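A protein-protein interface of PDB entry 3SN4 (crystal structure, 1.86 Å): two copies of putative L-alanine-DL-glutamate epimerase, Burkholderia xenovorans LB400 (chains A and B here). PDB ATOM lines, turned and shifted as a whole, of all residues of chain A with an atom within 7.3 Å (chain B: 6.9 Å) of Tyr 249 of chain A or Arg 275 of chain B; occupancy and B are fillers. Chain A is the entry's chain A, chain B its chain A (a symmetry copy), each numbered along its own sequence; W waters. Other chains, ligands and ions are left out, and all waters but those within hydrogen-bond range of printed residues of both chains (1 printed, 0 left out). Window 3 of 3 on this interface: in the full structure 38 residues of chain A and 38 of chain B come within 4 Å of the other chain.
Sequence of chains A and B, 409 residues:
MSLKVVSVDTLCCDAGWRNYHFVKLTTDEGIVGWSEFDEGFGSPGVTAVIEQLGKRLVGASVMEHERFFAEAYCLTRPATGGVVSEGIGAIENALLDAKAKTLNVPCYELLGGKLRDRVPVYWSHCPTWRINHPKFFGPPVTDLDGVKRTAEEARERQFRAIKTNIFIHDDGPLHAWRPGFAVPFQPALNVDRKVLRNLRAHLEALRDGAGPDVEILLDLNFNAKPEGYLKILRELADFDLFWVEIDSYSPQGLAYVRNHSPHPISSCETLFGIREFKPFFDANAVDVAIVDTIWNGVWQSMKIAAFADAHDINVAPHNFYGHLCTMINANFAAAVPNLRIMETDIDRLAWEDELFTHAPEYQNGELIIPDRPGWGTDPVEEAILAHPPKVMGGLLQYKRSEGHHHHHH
3 positions are printed for both chains. Of the 8 pairs that touch across the chains among the printed residues, none has its exchanged pair printed and touching as well.
Of the 17 printed residues of chain A, 4 touch a printed residue of chain B. Hydrophobic or aromatic side chains of chain A within 4 Å of the printed part of chain B: Phe 222, Tyr 249 and Trp 295. Of the 17 printed residues of chain B, 5 touch a printed residue of chain A.
CB of Phe 222 of chain A touches CD of Arg 77 of chain B (3.4 Å). Tyr 249 of chain A touches Tyr 73 of chain B. CE2 of Tyr 249 of chain A touches CG2 of Thr 80 of chain B (3.7 Å). Tyr 249 of chain A touches Arg 275 of chain B. Thr 270 of chain A touches Pro 78 of chain B. Trp 295 of chain A touches Pro 78 of chain B (CZ3 to O, 3.4 Å).
Of the printed residues of chain B, Phe 222 of chain A touches Arg 77. Of chain B, only Tyr 73 (3.7 Å), Arg 77 (2.8 Å), Pro 78 (3.3 Å), Thr 80 (3.7 Å) and Arg 275 (3.6 Å) come within 4 Å of Tyr 249 of chain A. Ala 79 of chain B touches none of the printed residues of chain A. Printed residues of chain A within 4 Å of Thr 80 of chain B: Tyr 249. Of chain A, only Tyr 249 comes within 4 Å of Arg 275 of chain B. The nearest residue of chain B that does not touch Tyr 249 of chain A is Ala 79 of chain B (4.5 Å). The nearest residue of chain A that does not touch Arg 275 of chain B is Ser 250 of chain A (4.1 Å).
The side-chain hydroxyl (OH) of Tyr 249 of chain A sits at hydrogen-bond distance from the backbone carbonyl oxygen (O) of Arg 77 of chain B. The backbone carbonyl oxygen (O) of Pro 78 of chain B lies within hydrogen-bond range of the side-chain hydroxyl (OH) of Tyr 249 of chain A (3.3 Å).
The side-chain hydroxyl (OG1) of Thr 270 of chain A sits at hydrogen-bond distance from the side-chain hydroxyl (OH) of Tyr 249 of chain A, at 3.3 Å.
Water W1 bridges the side-chain amide oxygen of Gln 252 of chain A (2.7 Å) and the side-chain amino group of Lys 278 of chain B (2.8 Å).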
ATOM      1  N   PHE A 222      -5.293  -2.747 -14.465  1.00  0.00           N
ATOM      2  CA  PHE A 222      -4.917  -1.574 -13.669  1.00  0.00           C
ATOM      3  C   PHE A 222      -6.146  -0.993 -12.926  1.00  0.00           C
ATOM      4  O   PHE A 222      -6.210   0.230 -12.679  1.00  0.00           O
ATOM      5  CB  PHE A 222      -4.360  -0.452 -14.563  1.00  0.00           C
ATOM      6  CG  PHE A 222      -3.015  -0.731 -15.208  1.00  0.00           C
ATOM      7  CD1 PHE A 222      -1.827  -0.305 -14.587  1.00  0.00           C
ATOM      8  CD2 PHE A 222      -2.938  -1.297 -16.479  1.00  0.00           C
ATOM      9  CE1 PHE A 222      -0.569  -0.496 -15.200  1.00  0.00           C
ATOM     10  CE2 PHE A 222      -1.699  -1.501 -17.103  1.00  0.00           C
ATOM     11  CZ  PHE A 222      -0.498  -1.077 -16.464  1.00  0.00           C
ATOM     12  N   LYS A 225      -6.151   0.504  -6.788  1.00  0.00           N
ATOM     13  CA  LYS A 225      -4.909   0.778  -6.055  1.00  0.00           C
ATOM     14  C   LYS A 225      -4.666  -0.418  -5.103  1.00  0.00           C
ATOM     15  O   LYS A 225      -5.594  -1.195  -4.825  1.00  0.00           O
ATOM     16  CB  LYS A 225      -5.006   2.085  -5.249  1.00  0.00           C
ATOM     17  CG  LYS A 225      -5.499   3.369  -5.992  1.00  0.00           C
ATOM     18  CD  LYS A 225      -4.607   3.769  -7.154  1.00  0.00           C
ATOM     19  CE  LYS A 225      -5.192   4.882  -8.011  1.00  0.00           C
ATOM     20  NZ  LYS A 225      -5.026   6.224  -7.368  1.00  0.00           N
ATOM     21  N   ASP A 247      -1.778  -5.384 -12.804  1.00  0.00           N
ATOM     22  CA  ASP A 247      -0.768  -4.493 -13.345  1.00  0.00           C
ATOM     23  C   ASP A 247      -0.557  -3.271 -12.465  1.00  0.00           C
ATOM     24  O   ASP A 247      -1.529  -2.661 -11.992  1.00  0.00           O
ATOM     25  CB  ASP A 247      -1.141  -4.056 -14.740  1.00  0.00           C
ATOM     26  CG  ASP A 247      -1.255  -5.211 -15.684  1.00  0.00           C
ATOM     27  OD1 ASP A 247      -0.280  -5.994 -15.821  1.00  0.00           O
ATOM     28  OD2 ASP A 247      -2.335  -5.316 -16.283  1.00  0.00           O
ATOM     29  N   SER A 248       0.704  -2.903 -12.275  1.00  0.00           N
ATOM     30  CA  SER A 248       1.084  -1.863 -11.324  1.00  0.00           C
ATOM     31  C   SER A 248       2.410  -1.292 -11.708  1.00  0.00           C
ATOM     32  O   SER A 248       3.307  -2.037 -12.135  1.00  0.00           O
ATOM     33  CB  SER A 248       1.200  -2.423  -9.894  1.00  0.00           C
ATOM     34  OG  SER A 248       1.629  -1.388  -9.010  1.00  0.00           O
ATOM     35  N   TYR A 249       2.544   0.020 -11.558  1.00  0.00           N
ATOM     36  CA  TYR A 249       3.842   0.686 -11.686  1.00  0.00           C
ATOM     37  C   TYR A 249       4.464   0.962 -10.333  1.00  0.00           C
ATOM     38  O   TYR A 249       5.374   1.792 -10.215  1.00  0.00           O
ATOM     39  CB  TYR A 249       3.713   1.938 -12.509  1.00  0.00           C
ATOM     40  CG  TYR A 249       3.318   1.631 -13.927  1.00  0.00           C
ATOM     41  CD1 TYR A 249       4.036   0.698 -14.677  1.00  0.00           C
ATOM     42  CD2 TYR A 249       2.217   2.236 -14.511  1.00  0.00           C
ATOM     43  CE1 TYR A 249       3.668   0.404 -15.986  1.00  0.00           C
ATOM     44  CE2 TYR A 249       1.849   1.957 -15.835  1.00  0.00           C
ATOM     45  CZ  TYR A 249       2.566   1.035 -16.554  1.00  0.00           C
ATOM     46  OH  TYR A 249       2.212   0.768 -17.864  1.00  0.00           O
ATOM     47  N   SER A 250       3.984   0.219  -9.335  1.00  0.00           N
ATOM     48  CA  SER A 250       4.507   0.288  -7.973  1.00  0.00           C
ATOM     49  C   SER A 250       4.943  -1.112  -7.525  1.00  0.00           C
ATOM     50  O   SER A 250       4.138  -1.895  -7.020  1.00  0.00           O
ATOM     51  CB  SER A 250       3.474   0.846  -7.010  1.00  0.00           C
ATOM     52  OG  SER A 250       4.009   0.877  -5.684  1.00  0.00           O
ATOM     53  N   PRO A 251       6.218  -1.436  -7.720  1.00  0.00           N
ATOM     54  CA  PRO A 251       6.739  -2.696  -7.225  1.00  0.00           C
ATOM     55  C   PRO A 251       6.490  -2.887  -5.713  1.00  0.00           C
ATOM     56  O   PRO A 251       6.101  -3.980  -5.287  1.00  0.00           O
ATOM     57  CB  PRO A 251       8.246  -2.585  -7.510  1.00  0.00           C
ATOM     58  CG  PRO A 251       8.403  -1.545  -8.516  1.00  0.00           C
ATOM     59  CD  PRO A 251       7.243  -0.634  -8.413  1.00  0.00           C
ATOM     60  N   GLN A 252       6.702  -1.828  -4.921  1.00  0.00           N
ATOM     61  CA  GLN A 252       6.477  -1.840  -3.465  1.00  0.00           C
ATOM     62  C   GLN A 252       5.033  -2.178  -3.144  1.00  0.00           C
ATOM     63  O   GLN A 252       4.725  -2.987  -2.255  1.00  0.00           O
ATOM     64  CB  GLN A 252       6.823  -0.465  -2.843  1.00  0.00           C
ATOM     65  CG  GLN A 252       6.925  -0.474  -1.314  1.00  0.00           C
ATOM     66  CD  GLN A 252       7.065   0.937  -0.675  1.00  0.00           C
ATOM     67  OE1 GLN A 252       7.312   1.937  -1.352  1.00  0.00           O
ATOM     68  NE2 GLN A 252       6.878   1.000   0.627  1.00  0.00           N
ATOM     69  N   GLY A 253       4.137  -1.510  -3.842  1.00  0.00           N
ATOM     70  CA  GLY A 253       2.709  -1.731  -3.641  1.00  0.00           C
ATOM     71  C   GLY A 253       2.297  -3.137  -4.050  1.00  0.00           C
ATOM     72  O   GLY A 253       1.609  -3.826  -3.312  1.00  0.00           O
ATOM     73  N   LEU A 254       2.717  -3.567  -5.235  1.00  0.00           N
ATOM     74  CA  LEU A 254       2.371  -4.911  -5.703  1.00  0.00           C
ATOM     75  C   LEU A 254       2.913  -6.002  -4.760  1.00  0.00           C
ATOM     76  O   LEU A 254       2.221  -6.986  -4.487  1.00  0.00           O
ATOM     77  CB  LEU A 254       2.876  -5.167  -7.129  1.00  0.00           C
ATOM     78  CG  LEU A 254       2.396  -6.518  -7.710  1.00  0.00           C
ATOM     79  CD1 LEU A 254       0.854  -6.658  -7.704  1.00  0.00           C
ATOM     80  CD2 LEU A 254       3.002  -6.707  -9.131  1.00  0.00           C
ATOM     81  N   SER A 267       1.865 -10.493 -13.043  1.00  0.00           N
ATOM     82  CA  SER A 267       1.925  -9.094 -13.486  1.00  0.00           C
ATOM     83  C   SER A 267       2.986  -8.982 -14.568  1.00  0.00           C
ATOM     84  O   SER A 267       3.529  -9.992 -15.003  1.00  0.00           O
ATOM     85  CB  SER A 267       2.290  -8.162 -12.308  1.00  0.00           C
ATOM     86  OG  SER A 267       2.140  -6.771 -12.634  1.00  0.00           O
ATOM     87  N   THR A 270       2.983  -5.172 -19.273  1.00  0.00           N
ATOM     88  CA  THR A 270       3.234  -3.901 -19.938  1.00  0.00           C
ATOM     89  C   THR A 270       4.674  -3.453 -19.826  1.00  0.00           C
ATOM     90  O   THR A 270       4.984  -2.347 -20.237  1.00  0.00           O
ATOM     91  CB  THR A 270       2.291  -2.749 -19.401  1.00  0.00           C
ATOM     92  OG1 THR A 270       2.582  -2.466 -18.032  1.00  0.00           O
ATOM     93  CG2 THR A 270       0.815  -3.120 -19.565  1.00  0.00           C
ATOM     94  N   LEU A 271       5.562  -4.285 -19.296  1.00  0.00           N
ATOM     95  CA  LEU A 271       6.911  -3.851 -19.006  1.00  0.00           C
ATOM     96  C   LEU A 271       7.887  -4.194 -20.115  1.00  0.00           C
ATOM     97  O   LEU A 271       7.714  -5.204 -20.823  1.00  0.00           O
ATOM     98  CB  LEU A 271       7.388  -4.497 -17.719  1.00  0.00           C
ATOM     99  CG  LEU A 271       6.590  -4.218 -16.460  1.00  0.00           C
ATOM    100  CD1 LEU A 271       7.345  -4.836 -15.271  1.00  0.00           C
ATOM    101  CD2 LEU A 271       6.375  -2.730 -16.262  1.00  0.00           C
ATOM    102  N   PHE A 272       8.939  -3.379 -20.213  1.00  0.00           N
ATOM    103  CA  PHE A 272       9.982  -3.514 -21.251  1.00  0.00           C
ATOM    104  C   PHE A 272      11.390  -3.748 -20.709  1.00  0.00           C
ATOM    105  O   PHE A 272      11.937  -2.906 -19.995  1.00  0.00           O
ATOM    106  CB  PHE A 272      10.049  -2.243 -22.107  1.00  0.00           C
ATOM    107  CG  PHE A 272       8.791  -1.951 -22.894  1.00  0.00           C
ATOM    108  CD1 PHE A 272       8.679  -2.345 -24.214  1.00  0.00           C
ATOM    109  CD2 PHE A 272       7.735  -1.250 -22.312  1.00  0.00           C
ATOM    110  CE1 PHE A 272       7.534  -2.056 -24.920  1.00  0.00           C
ATOM    111  CE2 PHE A 272       6.590  -0.983 -23.022  1.00  0.00           C
ATOM    112  CZ  PHE A 272       6.501  -1.381 -24.323  1.00  0.00           C
ATOM    113  N   GLU A 276      13.056  -3.021 -16.548  1.00  0.00           N
ATOM    114  CA  GLU A 276      11.776  -2.687 -15.923  1.00  0.00           C
ATOM    115  C   GLU A 276      11.231  -3.803 -15.055  1.00  0.00           C
ATOM    116  O   GLU A 276      10.441  -3.567 -14.117  1.00  0.00           O
ATOM    117  CB  GLU A 276      10.745  -2.283 -16.964  1.00  0.00           C
ATOM    118  CG  GLU A 276      11.011  -0.867 -17.497  1.00  0.00           C
ATOM    119  CD  GLU A 276       9.998  -0.389 -18.505  1.00  0.00           C
ATOM    120  OE1 GLU A 276       8.960  -1.088 -18.725  1.00  0.00           O
ATOM    121  OE2 GLU A 276      10.239   0.714 -19.065  1.00  0.00           O
ATOM    122  N   PHE A 280      10.487  -5.280  -9.748  1.00  0.00           N
ATOM    123  CA  PHE A 280       9.427  -6.206  -9.350  1.00  0.00           C
ATOM    124  C   PHE A 280       9.968  -7.497  -8.777  1.00  0.00           C
ATOM    125  O   PHE A 280       9.486  -7.974  -7.745  1.00  0.00           O
ATOM    126  CB  PHE A 280       8.491  -6.495 -10.515  1.00  0.00           C
ATOM    127  CG  PHE A 280       7.720  -5.304 -10.923  1.00  0.00           C
ATOM    128  CD1 PHE A 280       6.489  -5.029 -10.337  1.00  0.00           C
ATOM    129  CD2 PHE A 280       8.267  -4.380 -11.812  1.00  0.00           C
ATOM    130  CE1 PHE A 280       5.778  -3.866 -10.682  1.00  0.00           C
ATOM    131  CE2 PHE A 280       7.580  -3.247 -12.182  1.00  0.00           C
ATOM    132  CZ  PHE A 280       6.331  -2.968 -11.607  1.00  0.00           C
ATOM    133  N   TRP A 295       5.357  -6.700 -27.971  1.00  0.00           N
ATOM    134  CA  TRP A 295       5.904  -5.421 -27.582  1.00  0.00           C
ATOM    135  C   TRP A 295       7.437  -5.389 -27.501  1.00  0.00           C
ATOM    136  O   TRP A 295       8.093  -4.456 -28.020  1.00  0.00           O
ATOM    137  CB  TRP A 295       5.329  -5.063 -26.197  1.00  0.00           C
ATOM    138  CG  TRP A 295       3.998  -4.475 -26.246  1.00  0.00           C
ATOM    139  CD1 TRP A 295       3.049  -4.607 -27.243  1.00  0.00           C
ATOM    140  CD2 TRP A 295       3.440  -3.622 -25.268  1.00  0.00           C
ATOM    141  NE1 TRP A 295       1.929  -3.883 -26.909  1.00  0.00           N
ATOM    142  CE2 TRP A 295       2.143  -3.273 -25.702  1.00  0.00           C
ATOM    143  CE3 TRP A 295       3.905  -3.119 -24.050  1.00  0.00           C
ATOM    144  CZ2 TRP A 295       1.321  -2.409 -24.976  1.00  0.00           C
ATOM    145  CZ3 TRP A 295       3.073  -2.278 -23.328  1.00  0.00           C
ATOM    146  CH2 TRP A 295       1.805  -1.928 -23.799  1.00  0.00           C
ATOM    147  N   TYR B  73      -4.094   9.589 -19.127  1.00  0.00           N
ATOM    148  CA  TYR B  73      -3.256   8.638 -18.454  1.00  0.00           C
ATOM    149  C   TYR B  73      -3.940   7.291 -18.385  1.00  0.00           C
ATOM    150  O   TYR B  73      -3.271   6.287 -18.615  1.00  0.00           O
ATOM    151  CB  TYR B  73      -2.892   9.134 -17.038  1.00  0.00           C
ATOM    152  CG  TYR B  73      -1.965   8.191 -16.305  1.00  0.00           C
ATOM    153  CD1 TYR B  73      -0.608   8.127 -16.617  1.00  0.00           C
ATOM    154  CD2 TYR B  73      -2.452   7.326 -15.331  1.00  0.00           C
ATOM    155  CE1 TYR B  73       0.233   7.217 -15.967  1.00  0.00           C
ATOM    156  CE2 TYR B  73      -1.622   6.430 -14.679  1.00  0.00           C
ATOM    157  CZ  TYR B  73      -0.289   6.373 -15.005  1.00  0.00           C
ATOM    158  OH  TYR B  73       0.513   5.470 -14.345  1.00  0.00           O
ATOM    159  N   THR B  76      -4.032   5.614 -21.977  1.00  0.00           N
ATOM    160  CA  THR B  76      -2.725   5.181 -22.477  1.00  0.00           C
ATOM    161  C   THR B  76      -1.861   4.483 -21.412  1.00  0.00           C
ATOM    162  O   THR B  76      -0.631   4.323 -21.595  1.00  0.00           O
ATOM    163  CB  THR B  76      -1.934   6.363 -23.096  1.00  0.00           C
ATOM    164  OG1 THR B  76      -1.664   7.340 -22.097  1.00  0.00           O
ATOM    165  CG2 THR B  76      -2.709   7.016 -24.240  1.00  0.00           C
ATOM    166  N   ARG B  77      -2.492   4.062 -20.313  1.00  0.00           N
ATOM    167  CA  ARG B  77      -1.778   3.516 -19.138  1.00  0.00           C
ATOM    168  C   ARG B  77      -0.747   2.413 -19.496  1.00  0.00           C
ATOM    169  O   ARG B  77       0.358   2.466 -19.014  1.00  0.00           O
ATOM    170  CB  ARG B  77      -2.789   2.961 -18.136  1.00  0.00           C
ATOM    171  CG  ARG B  77      -2.481   3.220 -16.666  1.00  0.00           C
ATOM    172  CD  ARG B  77      -3.604   2.648 -15.793  1.00  0.00           C
ATOM    173  NE  ARG B  77      -3.524   3.220 -14.459  1.00  0.00           N
ATOM    174  CZ  ARG B  77      -4.343   4.111 -13.930  1.00  0.00           C
ATOM    175  NH1 ARG B  77      -5.428   4.522 -14.550  1.00  0.00           N
ATOM    176  NH2 ARG B  77      -4.078   4.558 -12.714  1.00  0.00           N
ATOM    177  N   PRO B  78      -1.115   1.437 -20.356  1.00  0.00           N
ATOM    178  CA  PRO B  78      -0.169   0.375 -20.687  1.00  0.00           C
ATOM    179  C   PRO B  78       1.133   0.811 -21.331  1.00  0.00           C
ATOM    180  O   PRO B  78       2.177   0.141 -21.122  1.00  0.00           O
ATOM    181  CB  PRO B  78      -0.966  -0.526 -21.627  1.00  0.00           C
ATOM    182  CG  PRO B  78      -2.339  -0.279 -21.268  1.00  0.00           C
ATOM    183  CD  PRO B  78      -2.419   1.164 -20.977  1.00  0.00           C
ATOM    184  N   ALA B  79       1.111   1.914 -22.070  1.00  0.00           N
ATOM    185  CA  ALA B  79       2.306   2.372 -22.781  1.00  0.00           C
ATOM    186  C   ALA B  79       2.745   3.765 -22.309  1.00  0.00           C
ATOM    187  O   ALA B  79       3.327   4.538 -23.064  1.00  0.00           O
ATOM    188  CB  ALA B  79       2.055   2.337 -24.305  1.00  0.00           C
ATOM    189  N   THR B  80       2.478   4.066 -21.043  1.00  0.00           N
ATOM    190  CA  THR B  80       2.833   5.360 -20.479  1.00  0.00           C
ATOM    191  C   THR B  80       4.340   5.565 -20.456  1.00  0.00           C
ATOM    192  O   THR B  80       5.145   4.609 -20.529  1.00  0.00           O
ATOM    193  CB  THR B  80       2.238   5.585 -19.058  1.00  0.00           C
ATOM    194  OG1 THR B  80       2.294   6.988 -18.730  1.00  0.00           O
ATOM    195  CG2 THR B  80       2.993   4.764 -18.003  1.00  0.00           C
ATOM    196  N   PHE B 272      10.041  10.839 -16.566  1.00  0.00           N
ATOM    197  CA  PHE B 272       8.623  11.247 -16.475  1.00  0.00           C
ATOM    198  C   PHE B 272       7.958  10.940 -15.135  1.00  0.00           C
ATOM    199  O   PHE B 272       7.851   9.779 -14.737  1.00  0.00           O
ATOM    200  CB  PHE B 272       7.795  10.530 -17.547  1.00  0.00           C
ATOM    201  CG  PHE B 272       8.179  10.872 -18.969  1.00  0.00           C
ATOM    202  CD1 PHE B 272       7.492  11.846 -19.670  1.00  0.00           C
ATOM    203  CD2 PHE B 272       9.212  10.188 -19.611  1.00  0.00           C
ATOM    204  CE1 PHE B 272       7.845  12.132 -20.968  1.00  0.00           C
ATOM    205  CE2 PHE B 272       9.566  10.496 -20.902  1.00  0.00           C
ATOM    206  CZ  PHE B 272       8.874  11.460 -21.573  1.00  0.00           C
ATOM    207  N   GLY B 273       7.465  11.980 -14.464  1.00  0.00           N
ATOM    208  CA  GLY B 273       6.653  11.832 -13.260  1.00  0.00           C
ATOM    209  C   GLY B 273       7.448  11.569 -12.008  1.00  0.00           C
ATOM    210  O   GLY B 273       8.572  11.110 -12.075  1.00  0.00           O
ATOM    211  N   ILE B 274       6.858  11.893 -10.859  1.00  0.00           N
ATOM    212  CA  ILE B 274       7.432  11.508  -9.567  1.00  0.00           C
ATOM    213  C   ILE B 274       7.931  10.048  -9.581  1.00  0.00           C
ATOM    214  O   ILE B 274       9.041   9.758  -9.099  1.00  0.00           O
ATOM    215  CB  ILE B 274       6.445  11.727  -8.400  1.00  0.00           C
ATOM    216  CG1 ILE B 274       6.169  13.244  -8.241  1.00  0.00           C
ATOM    217  CG2 ILE B 274       7.019  11.036  -7.101  1.00  0.00           C
ATOM    218  CD1 ILE B 274       5.256  13.689  -7.033  1.00  0.00           C
ATOM    219  N   ARG B 275       7.126   9.155 -10.161  1.00  0.00           N
ATOM    220  CA  ARG B 275       7.430   7.726 -10.245  1.00  0.00           C
ATOM    221  C   ARG B 275       8.828   7.425 -10.771  1.00  0.00           C
ATOM    222  O   ARG B 275       9.526   6.587 -10.210  1.00  0.00           O
ATOM    223  CB  ARG B 275       6.434   7.000 -11.146  1.00  0.00           C
ATOM    224  CG  ARG B 275       5.369   6.264 -10.399  1.00  0.00           C
ATOM    225  CD  ARG B 275       4.492   5.469 -11.342  1.00  0.00           C
ATOM    226  NE  ARG B 275       3.098   5.783 -11.072  1.00  0.00           N
ATOM    227  CZ  ARG B 275       2.299   5.150 -10.218  1.00  0.00           C
ATOM    228  NH1 ARG B 275       2.687   4.060  -9.514  1.00  0.00           N
ATOM    229  NH2 ARG B 275       1.057   5.608 -10.105  1.00  0.00           N
ATOM    230  N   GLU B 276       9.236   8.075 -11.851  1.00  0.00           N
ATOM    231  CA  GLU B 276      10.530   7.730 -12.439  1.00  0.00           C
ATOM    232  C   GLU B 276      11.697   8.395 -11.736  1.00  0.00           C
ATOM    233  O   GLU B 276      12.842   7.900 -11.772  1.00  0.00           O
ATOM    234  CB  GLU B 276      10.563   8.051 -13.924  1.00  0.00           C
ATOM    235  CG  GLU B 276       9.764   7.023 -14.739  1.00  0.00           C
ATOM    236  CD  GLU B 276       9.791   7.262 -16.226  1.00  0.00           C
ATOM    237  OE1 GLU B 276      10.555   8.160 -16.699  1.00  0.00           O
ATOM    238  OE2 GLU B 276       9.051   6.521 -16.928  1.00  0.00           O
ATOM    239  N   PHE B 277      11.405   9.524 -11.099  1.00  0.00           N
ATOM    240  CA  PHE B 277      12.423  10.278 -10.386  1.00  0.00           C
ATOM    241  C   PHE B 277      12.737   9.573  -9.065  1.00  0.00           C
ATOM    242  O   PHE B 277      13.878   9.602  -8.603  1.00  0.00           O
ATOM    243  CB  PHE B 277      11.964  11.727 -10.113  1.00  0.00           C
ATOM    244  CG  PHE B 277      12.226  12.682 -11.253  1.00  0.00           C
ATOM    245  CD1 PHE B 277      13.308  13.544 -11.219  1.00  0.00           C
ATOM    246  CD2 PHE B 277      11.363  12.753 -12.330  1.00  0.00           C
ATOM    247  CE1 PHE B 277      13.548  14.444 -12.255  1.00  0.00           C
ATOM    248  CE2 PHE B 277      11.586  13.651 -13.370  1.00  0.00           C
ATOM    249  CZ  PHE B 277      12.704  14.487 -13.331  1.00  0.00           C
ATOM    250  N   LYS B 278      11.726   8.953  -8.460  1.00  0.00           N
ATOM    251  CA  LYS B 278      11.867   8.371  -7.126  1.00  0.00           C
ATOM    252  C   LYS B 278      13.057   7.444  -6.896  1.00  0.00           C
ATOM    253  O   LYS B 278      13.764   7.605  -5.901  1.00  0.00           O
ATOM    254  CB  LYS B 278      10.581   7.662  -6.716  1.00  0.00           C
ATOM    255  CG  LYS B 278      10.610   7.045  -5.337  1.00  0.00           C
ATOM    256  CD  LYS B 278       9.202   6.581  -4.937  1.00  0.00           C
ATOM    257  CE  LYS B 278       9.265   5.249  -4.180  1.00  0.00           C
ATOM    258  NZ  LYS B 278      10.112   5.366  -2.957  1.00  0.00           N
ATOM    259  N   PRO B 279      13.294   6.464  -7.790  1.00  0.00           N
ATOM    260  CA  PRO B 279      14.411   5.568  -7.517  1.00  0.00           C
ATOM    261  C   PRO B 279      15.781   6.286  -7.496  1.00  0.00           C
ATOM    262  O   PRO B 279      16.677   5.876  -6.760  1.00  0.00           O
ATOM    263  CB  PRO B 279      14.364   4.541  -8.640  1.00  0.00           C
ATOM    264  CG  PRO B 279      13.211   4.822  -9.437  1.00  0.00           C
ATOM    265  CD  PRO B 279      12.592   6.126  -9.032  1.00  0.00           C
ATOM    266  N   PHE B 280      15.910   7.351  -8.263  1.00  0.00           N
ATOM    267  CA  PHE B 280      17.127   8.164  -8.266  1.00  0.00           C
ATOM    268  C   PHE B 280      17.324   8.917  -6.970  1.00  0.00           C
ATOM    269  O   PHE B 280      18.430   8.940  -6.422  1.00  0.00           O
ATOM    270  CB  PHE B 280      17.136   9.125  -9.446  1.00  0.00           C
ATOM    271  CG  PHE B 280      17.234   8.423 -10.741  1.00  0.00           C
ATOM    272  CD1 PHE B 280      18.478   8.139 -11.293  1.00  0.00           C
ATOM    273  CD2 PHE B 280      16.087   7.935 -11.367  1.00  0.00           C
ATOM    274  CE1 PHE B 280      18.576   7.422 -12.499  1.00  0.00           C
ATOM    275  CE2 PHE B 280      16.158   7.250 -12.557  1.00  0.00           C
ATOM    276  CZ  PHE B 280      17.408   6.970 -13.130  1.00  0.00           C
ATOM    277  N   ILE B 304       6.743  17.234  -9.581  1.00  0.00           N
ATOM    278  CA  ILE B 304       8.114  16.717  -9.522  1.00  0.00           C
ATOM    279  C   ILE B 304       9.025  17.688  -8.740  1.00  0.00           C
ATOM    280  O   ILE B 304       9.805  17.272  -7.883  1.00  0.00           O
ATOM    281  CB  ILE B 304       8.704  16.468 -10.921  1.00  0.00           C
ATOM    282  CG1 ILE B 304       7.872  15.457 -11.725  1.00  0.00           C
ATOM    283  CG2 ILE B 304      10.167  15.977 -10.803  1.00  0.00           C
ATOM    284  CD1 ILE B 304       8.261  15.366 -13.244  1.00  0.00           C
ATOM    285  N   PHE B 307       8.425  17.303  -5.037  1.00  0.00           N
ATOM    286  CA  PHE B 307       8.988  16.046  -4.567  1.00  0.00           C
ATOM    287  C   PHE B 307      10.502  16.239  -4.337  1.00  0.00           C
ATOM    288  O   PHE B 307      11.038  15.867  -3.317  1.00  0.00           O
ATOM    289  CB  PHE B 307       8.660  14.954  -5.622  1.00  0.00           C
ATOM    290  CG  PHE B 307       9.286  13.619  -5.381  1.00  0.00           C
ATOM    291  CD1 PHE B 307       9.061  12.928  -4.213  1.00  0.00           C
ATOM    292  CD2 PHE B 307      10.073  13.037  -6.353  1.00  0.00           C
ATOM    293  CE1 PHE B 307       9.636  11.714  -3.989  1.00  0.00           C
ATOM    294  CE2 PHE B 307      10.626  11.796  -6.159  1.00  0.00           C
ATOM    295  CZ  PHE B 307      10.414  11.136  -4.942  1.00  0.00           C
HETATM  296  O   HOH W   1       8.972   3.947  -0.809  1.00  0.00           O
